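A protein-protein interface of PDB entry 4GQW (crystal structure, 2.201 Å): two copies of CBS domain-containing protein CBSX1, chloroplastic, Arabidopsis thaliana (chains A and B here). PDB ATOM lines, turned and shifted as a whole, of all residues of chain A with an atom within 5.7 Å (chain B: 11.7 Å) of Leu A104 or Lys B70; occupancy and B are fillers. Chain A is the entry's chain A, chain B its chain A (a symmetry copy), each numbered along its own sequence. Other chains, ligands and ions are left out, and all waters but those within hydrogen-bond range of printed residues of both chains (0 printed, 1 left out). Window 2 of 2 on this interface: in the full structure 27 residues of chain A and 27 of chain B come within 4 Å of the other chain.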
ATOM      1  N   TYR A   5      15.349   8.414  14.953  1.00  0.00           N
ATOM      2  CA  TYR A   5      16.083   8.817  16.150  1.00  0.00           C
ATOM      3  C   TYR A   5      16.824   7.617  16.726  1.00  0.00           C
ATOM      4  O   TYR A   5      16.269   6.521  16.822  1.00  0.00           O
ATOM      5  CB  TYR A   5      15.147   9.397  17.216  1.00  0.00           C
ATOM      6  CG  TYR A   5      14.373  10.623  16.789  1.00  0.00           C
ATOM      7  CD1 TYR A   5      14.980  11.873  16.725  1.00  0.00           C
ATOM      8  CD2 TYR A   5      13.024  10.536  16.471  1.00  0.00           C
ATOM      9  CE1 TYR A   5      14.265  12.996  16.341  1.00  0.00           C
ATOM     10  CE2 TYR A   5      12.305  11.652  16.087  1.00  0.00           C
ATOM     11  CZ  TYR A   5      12.928  12.877  16.025  1.00  0.00           C
ATOM     12  OH  TYR A   5      12.208  13.985  15.644  1.00  0.00           O
ATOM     13  N   THR A   6      18.078   7.826  17.111  1.00  0.00           N
ATOM     14  CA  THR A   6      18.886   6.746  17.664  1.00  0.00           C
ATOM     15  C   THR A   6      19.266   6.984  19.123  1.00  0.00           C
ATOM     16  O   THR A   6      19.221   8.111  19.617  1.00  0.00           O
ATOM     17  CB  THR A   6      20.165   6.513  16.843  1.00  0.00           C
ATOM     18  OG1 THR A   6      20.956   7.706  16.838  1.00  0.00           O
ATOM     19  CG2 THR A   6      19.811   6.139  15.413  1.00  0.00           C
ATOM     20  N   VAL A   7      19.638   5.907  19.802  1.00  0.00           N
ATOM     21  CA  VAL A   7      20.010   5.956  21.210  1.00  0.00           C
ATOM     22  C   VAL A   7      21.248   6.820  21.421  1.00  0.00           C
ATOM     23  O   VAL A   7      21.338   7.572  22.390  1.00  0.00           O
ATOM     24  CB  VAL A   7      20.252   4.530  21.757  1.00  0.00           C
ATOM     25  CG1 VAL A   7      20.891   4.574  23.131  1.00  0.00           C
ATOM     26  CG2 VAL A   7      18.941   3.760  21.794  1.00  0.00           C
ATOM     27  N   PHE A  10      20.804  10.603  22.241  1.00  0.00           N
ATOM     28  CA  PHE A  10      20.228  11.103  23.484  1.00  0.00           C
ATOM     29  C   PHE A  10      20.767  10.430  24.741  1.00  0.00           C
ATOM     30  O   PHE A  10      20.328  10.736  25.848  1.00  0.00           O
ATOM     31  CB  PHE A  10      18.704  11.002  23.431  1.00  0.00           C
ATOM     32  CG  PHE A  10      18.086  11.838  22.350  1.00  0.00           C
ATOM     33  CD1 PHE A  10      17.851  13.187  22.552  1.00  0.00           C
ATOM     34  CD2 PHE A  10      17.753  11.278  21.128  1.00  0.00           C
ATOM     35  CE1 PHE A  10      17.288  13.961  21.561  1.00  0.00           C
ATOM     36  CE2 PHE A  10      17.187  12.046  20.133  1.00  0.00           C
ATOM     37  CZ  PHE A  10      16.954  13.390  20.349  1.00  0.00           C
ATOM     38  N   THR A 102      20.887   1.875  17.779  1.00  0.00           N
ATOM     39  CA  THR A 102      19.583   1.381  18.194  1.00  0.00           C
ATOM     40  C   THR A 102      18.531   2.479  18.105  1.00  0.00           C
ATOM     41  O   THR A 102      18.763   3.615  18.522  1.00  0.00           O
ATOM     42  CB  THR A 102      19.633   0.830  19.632  1.00  0.00           C
ATOM     43  OG1 THR A 102      20.509  -0.302  19.676  1.00  0.00           O
ATOM     44  CG2 THR A 102      18.246   0.409  20.103  1.00  0.00           C
ATOM     45  N   ASN A 103      17.383   2.133  17.534  1.00  0.00           N
ATOM     46  CA  ASN A 103      16.263   3.053  17.452  1.00  0.00           C
ATOM     47  C   ASN A 103      15.827   3.489  18.843  1.00  0.00           C
ATOM     48  O   ASN A 103      15.716   2.671  19.755  1.00  0.00           O
ATOM     49  CB  ASN A 103      15.099   2.400  16.709  1.00  0.00           C
ATOM     50  CG  ASN A 103      13.915   3.326  16.550  1.00  0.00           C
ATOM     51  OD1 ASN A 103      14.024   4.541  16.731  1.00  0.00           O
ATOM     52  ND2 ASN A 103      12.768   2.755  16.200  1.00  0.00           N
ATOM     53  N   LEU A 104      15.588   4.786  18.996  1.00  0.00           N
ATOM     54  CA  LEU A 104      15.257   5.371  20.287  1.00  0.00           C
ATOM     55  C   LEU A 104      13.929   4.852  20.825  1.00  0.00           C
ATOM     56  O   LEU A 104      13.757   4.701  22.034  1.00  0.00           O
ATOM     57  CB  LEU A 104      15.207   6.894  20.169  1.00  0.00           C
ATOM     58  CG  LEU A 104      14.998   7.674  21.466  1.00  0.00           C
ATOM     59  CD1 LEU A 104      16.146   7.413  22.423  1.00  0.00           C
ATOM     60  CD2 LEU A 104      14.861   9.162  21.178  1.00  0.00           C
ATOM     61  N   GLU A 105      12.998   4.566  19.921  1.00  0.00           N
ATOM     62  CA  GLU A 105      11.661   4.137  20.316  1.00  0.00           C
ATOM     63  C   GLU A 105      11.625   2.740  20.930  1.00  0.00           C
ATOM     64  O   GLU A 105      10.770   2.454  21.766  1.00  0.00           O
ATOM     65  CB  GLU A 105      10.690   4.230  19.138  1.00  0.00           C
ATOM     66  CG  GLU A 105      10.249   5.648  18.836  1.00  0.00           C
ATOM     67  CD  GLU A 105       9.041   5.705  17.927  1.00  0.00           C
ATOM     68  OE1 GLU A 105       8.721   4.678  17.291  1.00  0.00           O
ATOM     69  OE2 GLU A 105       8.405   6.778  17.851  1.00  0.00           O
ATOM     70  N   ASP A 106      12.546   1.875  20.520  1.00  0.00           N
ATOM     71  CA  ASP A 106      12.643   0.541  21.105  1.00  0.00           C
ATOM     72  C   ASP A 106      13.174   0.630  22.534  1.00  0.00           C
ATOM     73  O   ASP A 106      12.630   0.013  23.464  1.00  0.00           O
ATOM     74  CB  ASP A 106      13.558  -0.347  20.263  1.00  0.00           C
ATOM     75  CG  ASP A 106      13.015  -0.586  18.871  1.00  0.00           C
ATOM     76  OD1 ASP A 106      11.778  -0.558  18.702  1.00  0.00           O
ATOM     77  OD2 ASP A 106      13.823  -0.810  17.947  1.00  0.00           O
ATOM     78  N   ALA A 107      14.241   1.408  22.696  1.00  0.00           N
ATOM     79  CA  ALA A 107      14.838   1.637  24.003  1.00  0.00           C
ATOM     80  C   ALA A 107      13.802   2.253  24.927  1.00  0.00           C
ATOM     81  O   ALA A 107      13.708   1.891  26.098  1.00  0.00           O
ATOM     82  CB  ALA A 107      16.043   2.547  23.878  1.00  0.00           C
ATOM     83  N   ALA A 108      13.014   3.173  24.380  1.00  0.00           N
ATOM     84  CA  ALA A 108      11.929   3.797  25.121  1.00  0.00           C
ATOM     85  C   ALA A 108      10.890   2.758  25.521  1.00  0.00           C
ATOM     86  O   ALA A 108      10.381   2.785  26.641  1.00  0.00           O
ATOM     87  CB  ALA A 108      11.288   4.898  24.293  1.00  0.00           C
ATOM     88  N   LYS A 109      10.580   1.844  24.605  1.00  0.00           N
ATOM     89  CA  LYS A 109       9.665   0.750  24.916  1.00  0.00           C
ATOM     90  C   LYS A 109      10.154  -0.020  26.131  1.00  0.00           C
ATOM     91  O   LYS A 109       9.376  -0.323  27.032  1.00  0.00           O
ATOM     92  CB  LYS A 109       9.516  -0.201  23.730  1.00  0.00           C
ATOM     93  CG  LYS A 109       8.645   0.332  22.614  1.00  0.00           C
ATOM     94  CD  LYS A 109       8.754  -0.541  21.381  1.00  0.00           C
ATOM     95  CE  LYS A 109       8.092   0.106  20.178  1.00  0.00           C
ATOM     96  NZ  LYS A 109       8.329  -0.689  18.946  1.00  0.00           N
ATOM     97  N   LEU A 112       9.941   2.058  29.437  1.00  0.00           N
ATOM     98  CA  LEU A 112       8.604   2.487  29.832  1.00  0.00           C
ATOM     99  C   LEU A 112       7.686   1.313  30.145  1.00  0.00           C
ATOM    100  O   LEU A 112       6.781   1.428  30.970  1.00  0.00           O
ATOM    101  CB  LEU A 112       7.979   3.366  28.751  1.00  0.00           C
ATOM    102  CG  LEU A 112       8.680   4.694  28.453  1.00  0.00           C
ATOM    103  CD1 LEU A 112       8.277   5.190  27.075  1.00  0.00           C
ATOM    104  CD2 LEU A 112       8.358   5.736  29.511  1.00  0.00           C
ATOM    105  N   ILE A 132      21.769   5.003  28.302  1.00  0.00           N
ATOM    106  CA  ILE A 132      20.491   5.643  28.010  1.00  0.00           C
ATOM    107  C   ILE A 132      19.518   5.464  29.173  1.00  0.00           C
ATOM    108  O   ILE A 132      19.246   4.344  29.606  1.00  0.00           O
ATOM    109  CB  ILE A 132      19.868   5.116  26.691  1.00  0.00           C
ATOM    110  CG1 ILE A 132      18.473   5.711  26.478  1.00  0.00           C
ATOM    111  CG2 ILE A 132      19.828   3.598  26.660  1.00  0.00           C
ATOM    112  CD1 ILE A 132      18.499   7.067  25.823  1.00  0.00           C
ATOM    113  N   VAL A 137      15.099   9.729  27.684  1.00  0.00           N
ATOM    114  CA  VAL A 137      13.975   9.554  26.776  1.00  0.00           C
ATOM    115  C   VAL A 137      12.991  10.698  26.932  1.00  0.00           C
ATOM    116  O   VAL A 137      12.507  11.246  25.940  1.00  0.00           O
ATOM    117  CB  VAL A 137      13.248   8.222  27.033  1.00  0.00           C
ATOM    118  CG1 VAL A 137      11.985   8.138  26.198  1.00  0.00           C
ATOM    119  CG2 VAL A 137      14.169   7.059  26.722  1.00  0.00           C
ATOM    120  N   ALA A 140      14.441  13.680  25.405  1.00  0.00           N
ATOM    121  CA  ALA A 140      14.366  13.523  23.961  1.00  0.00           C
ATOM    122  C   ALA A 140      12.982  13.907  23.462  1.00  0.00           C
ATOM    123  O   ALA A 140      12.842  14.537  22.415  1.00  0.00           O
ATOM    124  CB  ALA A 140      14.694  12.096  23.567  1.00  0.00           C
ATOM    125  N   ALA A 141      11.960  13.532  24.223  1.00  0.00           N
ATOM    126  CA  ALA A 141      10.597  13.908  23.882  1.00  0.00           C
ATOM    127  C   ALA A 141      10.382  15.407  24.072  1.00  0.00           C
ATOM    128  O   ALA A 141       9.537  16.008  23.413  1.00  0.00           O
ATOM    129  CB  ALA A 141       9.604  13.120  24.714  1.00  0.00           C
ATOM    130  N   LEU B  30       7.994  17.052  34.252  1.00  0.00           N
ATOM    131  CA  LEU B  30       8.957  16.281  33.477  1.00  0.00           C
ATOM    132  C   LEU B  30      10.167  17.132  33.122  1.00  0.00           C
ATOM    133  O   LEU B  30      11.308  16.671  33.203  1.00  0.00           O
ATOM    134  CB  LEU B  30       8.312  15.734  32.203  1.00  0.00           C
ATOM    135  CG  LEU B  30       7.263  14.633  32.379  1.00  0.00           C
ATOM    136  CD1 LEU B  30       6.684  14.234  31.030  1.00  0.00           C
ATOM    137  CD2 LEU B  30       7.864  13.428  33.083  1.00  0.00           C
ATOM    138  N   VAL B  34      14.089  16.538  34.069  1.00  0.00           N
ATOM    139  CA  VAL B  34      15.187  16.534  33.112  1.00  0.00           C
ATOM    140  C   VAL B  34      16.276  17.524  33.500  1.00  0.00           C
ATOM    141  O   VAL B  34      17.456  17.175  33.556  1.00  0.00           O
ATOM    142  CB  VAL B  34      14.691  16.863  31.691  1.00  0.00           C
ATOM    143  CG1 VAL B  34      15.859  17.197  30.781  1.00  0.00           C
ATOM    144  CG2 VAL B  34      13.879  15.705  31.134  1.00  0.00           C
ATOM    145  N   LEU B  59       4.109  10.192  36.564  1.00  0.00           N
ATOM    146  CA  LEU B  59       3.864  11.238  35.578  1.00  0.00           C
ATOM    147  C   LEU B  59       3.652  10.685  34.176  1.00  0.00           C
ATOM    148  O   LEU B  59       2.840  11.208  33.415  1.00  0.00           O
ATOM    149  CB  LEU B  59       5.022  12.232  35.576  1.00  0.00           C
ATOM    150  CG  LEU B  59       5.189  13.019  36.874  1.00  0.00           C
ATOM    151  CD1 LEU B  59       6.512  13.758  36.873  1.00  0.00           C
ATOM    152  CD2 LEU B  59       4.034  13.990  37.042  1.00  0.00           C
ATOM    153  N   LEU B  60       4.383   9.632  33.834  1.00  0.00           N
ATOM    154  CA  LEU B  60       4.256   9.035  32.513  1.00  0.00           C
ATOM    155  C   LEU B  60       3.171   7.970  32.516  1.00  0.00           C
ATOM    156  O   LEU B  60       2.837   7.411  31.470  1.00  0.00           O
ATOM    157  CB  LEU B  60       5.587   8.430  32.074  1.00  0.00           C
ATOM    158  CG  LEU B  60       6.782   9.384  32.065  1.00  0.00           C
ATOM    159  CD1 LEU B  60       8.064   8.618  31.792  1.00  0.00           C
ATOM    160  CD2 LEU B  60       6.580  10.470  31.028  1.00  0.00           C
ATOM    161  N   ALA B  61       2.628   7.706  33.702  1.00  0.00           N
ATOM    162  CA  ALA B  61       1.566   6.720  33.889  1.00  0.00           C
ATOM    163  C   ALA B  61       1.942   5.350  33.335  1.00  0.00           C
ATOM    164  O   ALA B  61       1.280   4.833  32.437  1.00  0.00           O
ATOM    165  CB  ALA B  61       0.266   7.209  33.262  1.00  0.00           C
ATOM    166  N   LEU B  62       3.006   4.764  33.874  1.00  0.00           N
ATOM    167  CA  LEU B  62       3.473   3.466  33.403  1.00  0.00           C
ATOM    168  C   LEU B  62       2.712   2.331  34.064  1.00  0.00           C
ATOM    169  O   LEU B  62       2.525   1.269  33.473  1.00  0.00           O
ATOM    170  CB  LEU B  62       4.963   3.306  33.678  1.00  0.00           C
ATOM    171  CG  LEU B  62       5.816   4.470  33.187  1.00  0.00           C
ATOM    172  CD1 LEU B  62       7.282   4.197  33.467  1.00  0.00           C
ATOM    173  CD2 LEU B  62       5.575   4.695  31.708  1.00  0.00           C
ATOM    174  N   THR B  68       2.426   1.527  26.394  1.00  0.00           N
ATOM    175  CA  THR B  68       3.085   2.796  26.673  1.00  0.00           C
ATOM    176  C   THR B  68       4.413   2.869  25.931  1.00  0.00           C
ATOM    177  O   THR B  68       5.216   1.939  25.994  1.00  0.00           O
ATOM    178  CB  THR B  68       3.357   2.970  28.176  1.00  0.00           C
ATOM    179  OG1 THR B  68       4.535   2.238  28.535  1.00  0.00           O
ATOM    180  CG2 THR B  68       2.178   2.471  28.997  1.00  0.00           C
ATOM    181  N   TRP B  69       4.642   3.974  25.230  1.00  0.00           N
ATOM    182  CA  TRP B  69       5.897   4.164  24.509  1.00  0.00           C
ATOM    183  C   TRP B  69       6.198   5.622  24.173  1.00  0.00           C
ATOM    184  O   TRP B  69       5.598   6.539  24.731  1.00  0.00           O
ATOM    185  CB  TRP B  69       5.947   3.293  23.252  1.00  0.00           C
ATOM    186  CG  TRP B  69       4.844   3.532  22.270  1.00  0.00           C
ATOM    187  CD1 TRP B  69       3.507   3.369  22.480  1.00  0.00           C
ATOM    188  CD2 TRP B  69       4.990   3.943  20.909  1.00  0.00           C
ATOM    189  NE1 TRP B  69       2.809   3.669  21.336  1.00  0.00           N
ATOM    190  CE2 TRP B  69       3.698   4.022  20.355  1.00  0.00           C
ATOM    191  CE3 TRP B  69       6.089   4.256  20.105  1.00  0.00           C
ATOM    192  CZ2 TRP B  69       3.475   4.402  19.034  1.00  0.00           C
ATOM    193  CZ3 TRP B  69       5.867   4.632  18.798  1.00  0.00           C
ATOM    194  CH2 TRP B  69       4.570   4.700  18.274  1.00  0.00           C
ATOM    195  N   LYS B  70       7.143   5.820  23.259  1.00  0.00           N
ATOM    196  CA  LYS B  70       7.691   7.142  22.986  1.00  0.00           C
ATOM    197  C   LYS B  70       6.654   8.123  22.464  1.00  0.00           C
ATOM    198  O   LYS B  70       6.600   9.274  22.901  1.00  0.00           O
ATOM    199  CB  LYS B  70       8.846   7.037  21.994  1.00  0.00           C
ATOM    200  CG  LYS B  70       9.450   8.370  21.615  1.00  0.00           C
ATOM    201  CD  LYS B  70      10.397   8.885  22.677  1.00  0.00           C
ATOM    202  CE  LYS B  70      10.833  10.286  22.329  1.00  0.00           C
ATOM    203  NZ  LYS B  70      11.276  10.346  20.913  1.00  0.00           N
ATOM    204  N   THR B  71       5.833   7.667  21.527  1.00  0.00           N
ATOM    205  CA  THR B  71       4.811   8.516  20.938  1.00  0.00           C
ATOM    206  C   THR B  71       3.714   8.829  21.954  1.00  0.00           C
ATOM    207  O   THR B  71       3.093   9.890  21.904  1.00  0.00           O
ATOM    208  CB  THR B  71       4.220   7.874  19.666  1.00  0.00           C
ATOM    209  OG1 THR B  71       5.266   7.690  18.705  1.00  0.00           O
ATOM    210  CG2 THR B  71       3.141   8.756  19.054  1.00  0.00           C
ATOM    211  N   PHE B  72       3.491   7.911  22.889  1.00  0.00           N
ATOM    212  CA  PHE B  72       2.539   8.159  23.962  1.00  0.00           C
ATOM    213  C   PHE B  72       3.009   9.322  24.826  1.00  0.00           C
ATOM    214  O   PHE B  72       2.197  10.091  25.333  1.00  0.00           O
ATOM    215  CB  PHE B  72       2.337   6.916  24.802  1.00  0.00           C
ATOM    216  N   ASN B  73       4.323   9.451  24.988  1.00  0.00           N
ATOM    217  CA  ASN B  73       4.890  10.584  25.711  1.00  0.00           C
ATOM    218  C   ASN B  73       4.850  11.859  24.870  1.00  0.00           C
ATOM    219  O   ASN B  73       4.525  12.936  25.382  1.00  0.00           O
ATOM    220  CB  ASN B  73       6.325  10.289  26.146  1.00  0.00           C
ATOM    221  CG  ASN B  73       6.438   9.018  26.953  1.00  0.00           C
ATOM    222  OD1 ASN B  73       5.493   8.612  27.628  1.00  0.00           O
ATOM    223  ND2 ASN B  73       7.598   8.380  26.887  1.00  0.00           N
ATOM    224  N   ALA B  74       5.192  11.724  23.586  1.00  0.00           N
ATOM    225  CA  ALA B  74       5.061  12.804  22.607  1.00  0.00           C
ATOM    226  C   ALA B  74       3.707  13.466  22.768  1.00  0.00           C
ATOM    227  O   ALA B  74       3.603  14.681  22.931  1.00  0.00           O
ATOM    228  CB  ALA B  74       5.131  12.244  21.185  1.00  0.00           C
ATOM    229  N   VAL B  75       2.674  12.633  22.727  1.00  0.00           N
ATOM    230  CA  VAL B  75       1.298  13.084  22.822  1.00  0.00           C
ATOM    231  C   VAL B  75       0.967  13.590  24.221  1.00  0.00           C
ATOM    232  O   VAL B  75       0.297  14.613  24.368  1.00  0.00           O
ATOM    233  CB  VAL B  75       0.324  11.952  22.435  1.00  0.00           C
ATOM    234  CG1 VAL B  75      -1.107  12.334  22.770  1.00  0.00           C
ATOM    235  CG2 VAL B  75       0.463  11.624  20.957  1.00  0.00           C
ATOM    236  N   GLN B  76       1.446  12.883  25.240  1.00  0.00           N
ATOM    237  CA  GLN B  76       1.166  13.247  26.627  1.00  0.00           C
ATOM    238  C   GLN B  76       1.627  14.664  26.923  1.00  0.00           C
ATOM    239  O   GLN B  76       0.985  15.389  27.682  1.00  0.00           O
ATOM    240  CB  GLN B  76       1.842  12.279  27.598  1.00  0.00           C
ATOM    241  CG  GLN B  76       1.547  12.566  29.066  1.00  0.00           C
ATOM    242  CD  GLN B  76       0.206  12.014  29.513  1.00  0.00           C
ATOM    243  OE1 GLN B  76      -0.293  11.038  28.950  1.00  0.00           O
ATOM    244  NE2 GLN B  76      -0.385  12.635  30.529  1.00  0.00           N
ATOM    245  N   LYS B  77       2.737  15.062  26.311  1.00  0.00           N
ATOM    246  CA  LYS B  77       3.275  16.399  26.523  1.00  0.00           C
ATOM    247  C   LYS B  77       2.572  17.452  25.666  1.00  0.00           C
ATOM    248  O   LYS B  77       3.141  18.502  25.373  1.00  0.00           O
ATOM    249  CB  LYS B  77       4.771  16.414  26.264  1.00  0.00           C
ATOM    250  N   LEU B  78       1.334  17.168  25.272  1.00  0.00           N
ATOM    251  CA  LEU B  78       0.546  18.097  24.467  1.00  0.00           C
ATOM    252  C   LEU B  78      -0.910  18.145  24.927  1.00  0.00           C
ATOM    253  O   LEU B  78      -1.517  17.113  25.214  1.00  0.00           O
ATOM    254  CB  LEU B  78       0.616  17.720  22.986  1.00  0.00           C
ATOM    255  CG  LEU B  78       1.951  17.956  22.278  1.00  0.00           C
ATOM    256  CD1 LEU B  78       1.930  17.347  20.887  1.00  0.00           C
ATOM    257  CD2 LEU B  78       2.259  19.441  22.204  1.00  0.00           C
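O of Leu A112 lies within hydrogen-bond range of OG1 of Thr B68.
The side-chain hydroxyl (OG1) of Thr B71 sits at hydrogen-bond distance from the side-chain carboxylate (OE2) of Glu A105, 3.4 Å away.
The side-chain amide oxygen (OD1) of Asn A103 lies close to the backbone NH (N) of Glu A105, 3.4 Å away.
The backbone NH of Leu A104 sits at hydrogen-bond distance from the backbone carbonyl oxygen of Tyr A5 (2.9 Å).
O of Trp B69 lies close to ND2 of Asn B73 (3.5 Å).
Among the printed residues, merely in contact across the chains: Leu A104 with Lys B70 (3.8 Å), Glu A105 with Trp B69 (3.2 Å), Glu A105 with Lys B70 (3.7 Å), Ala A108 with Lys B70 (3.98 Å), Leu A112 with Leu B60 (3.7 Å), Leu A112 with Leu B62 (3.6 Å), Leu A112 with Trp B69 (3.6 Å), Leu A112 with Asn B73 (3.3 Å), Val A137 with Lys B70 (3.9 Å) and Ala A141 with Lys B70 (3.9 Å).
No residue of chain B comes within 4 Å of Thr A6.
No residue of chain B comes within 4 Å of Val A7.
No residue of chain B comes within 4 Å of Phe A10.
No residue of chain B comes within 4 Å of Thr A102.
No residue of chain B comes within 4 Å of Asn A103.
Leu A104 touches just one residue of chain B: Lys B70.
Of the printed residues of chain B, Glu A105 touches Trp B69, Lys B70 and Thr B71.
Printed residues of chain B within 4 Å of Ala A108: Lys B70.
Of chain B, only Lys B70 comes within 4 Å of Ala A141.
Of the printed residues of chain A, Leu B60 touches Leu A112 (3.7 Å).
Printed residues of chain A within 4 Å of Thr B68: Leu A112.
Of the printed residues of chain A, Lys B70 touches Leu A104, Glu A105, Ala A108, Val A137 and Ala A141.
Gln B76 touches none of the printed residues of chain A.
The nearest printed residue of chain A that does not touch Leu B60 is Val A137 (6.8 Å).
Of the 17 printed residues of chain A, 6 touch a printed residue of chain B.
Printed residues of chain A that touch a printed residue of chain B: Leu A104, Glu A105, Ala A108, Leu A112, Val A137 and Ala A141.
Hydrophobic or aromatic side chains of chain B that line the printed part of chain A: Leu B60, Leu B62 and Trp B69.
No position is printed for both chains.
Of the 12 pairs that touch across the chains among the printed residues, none has its exchanged pair printed and touching as well.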
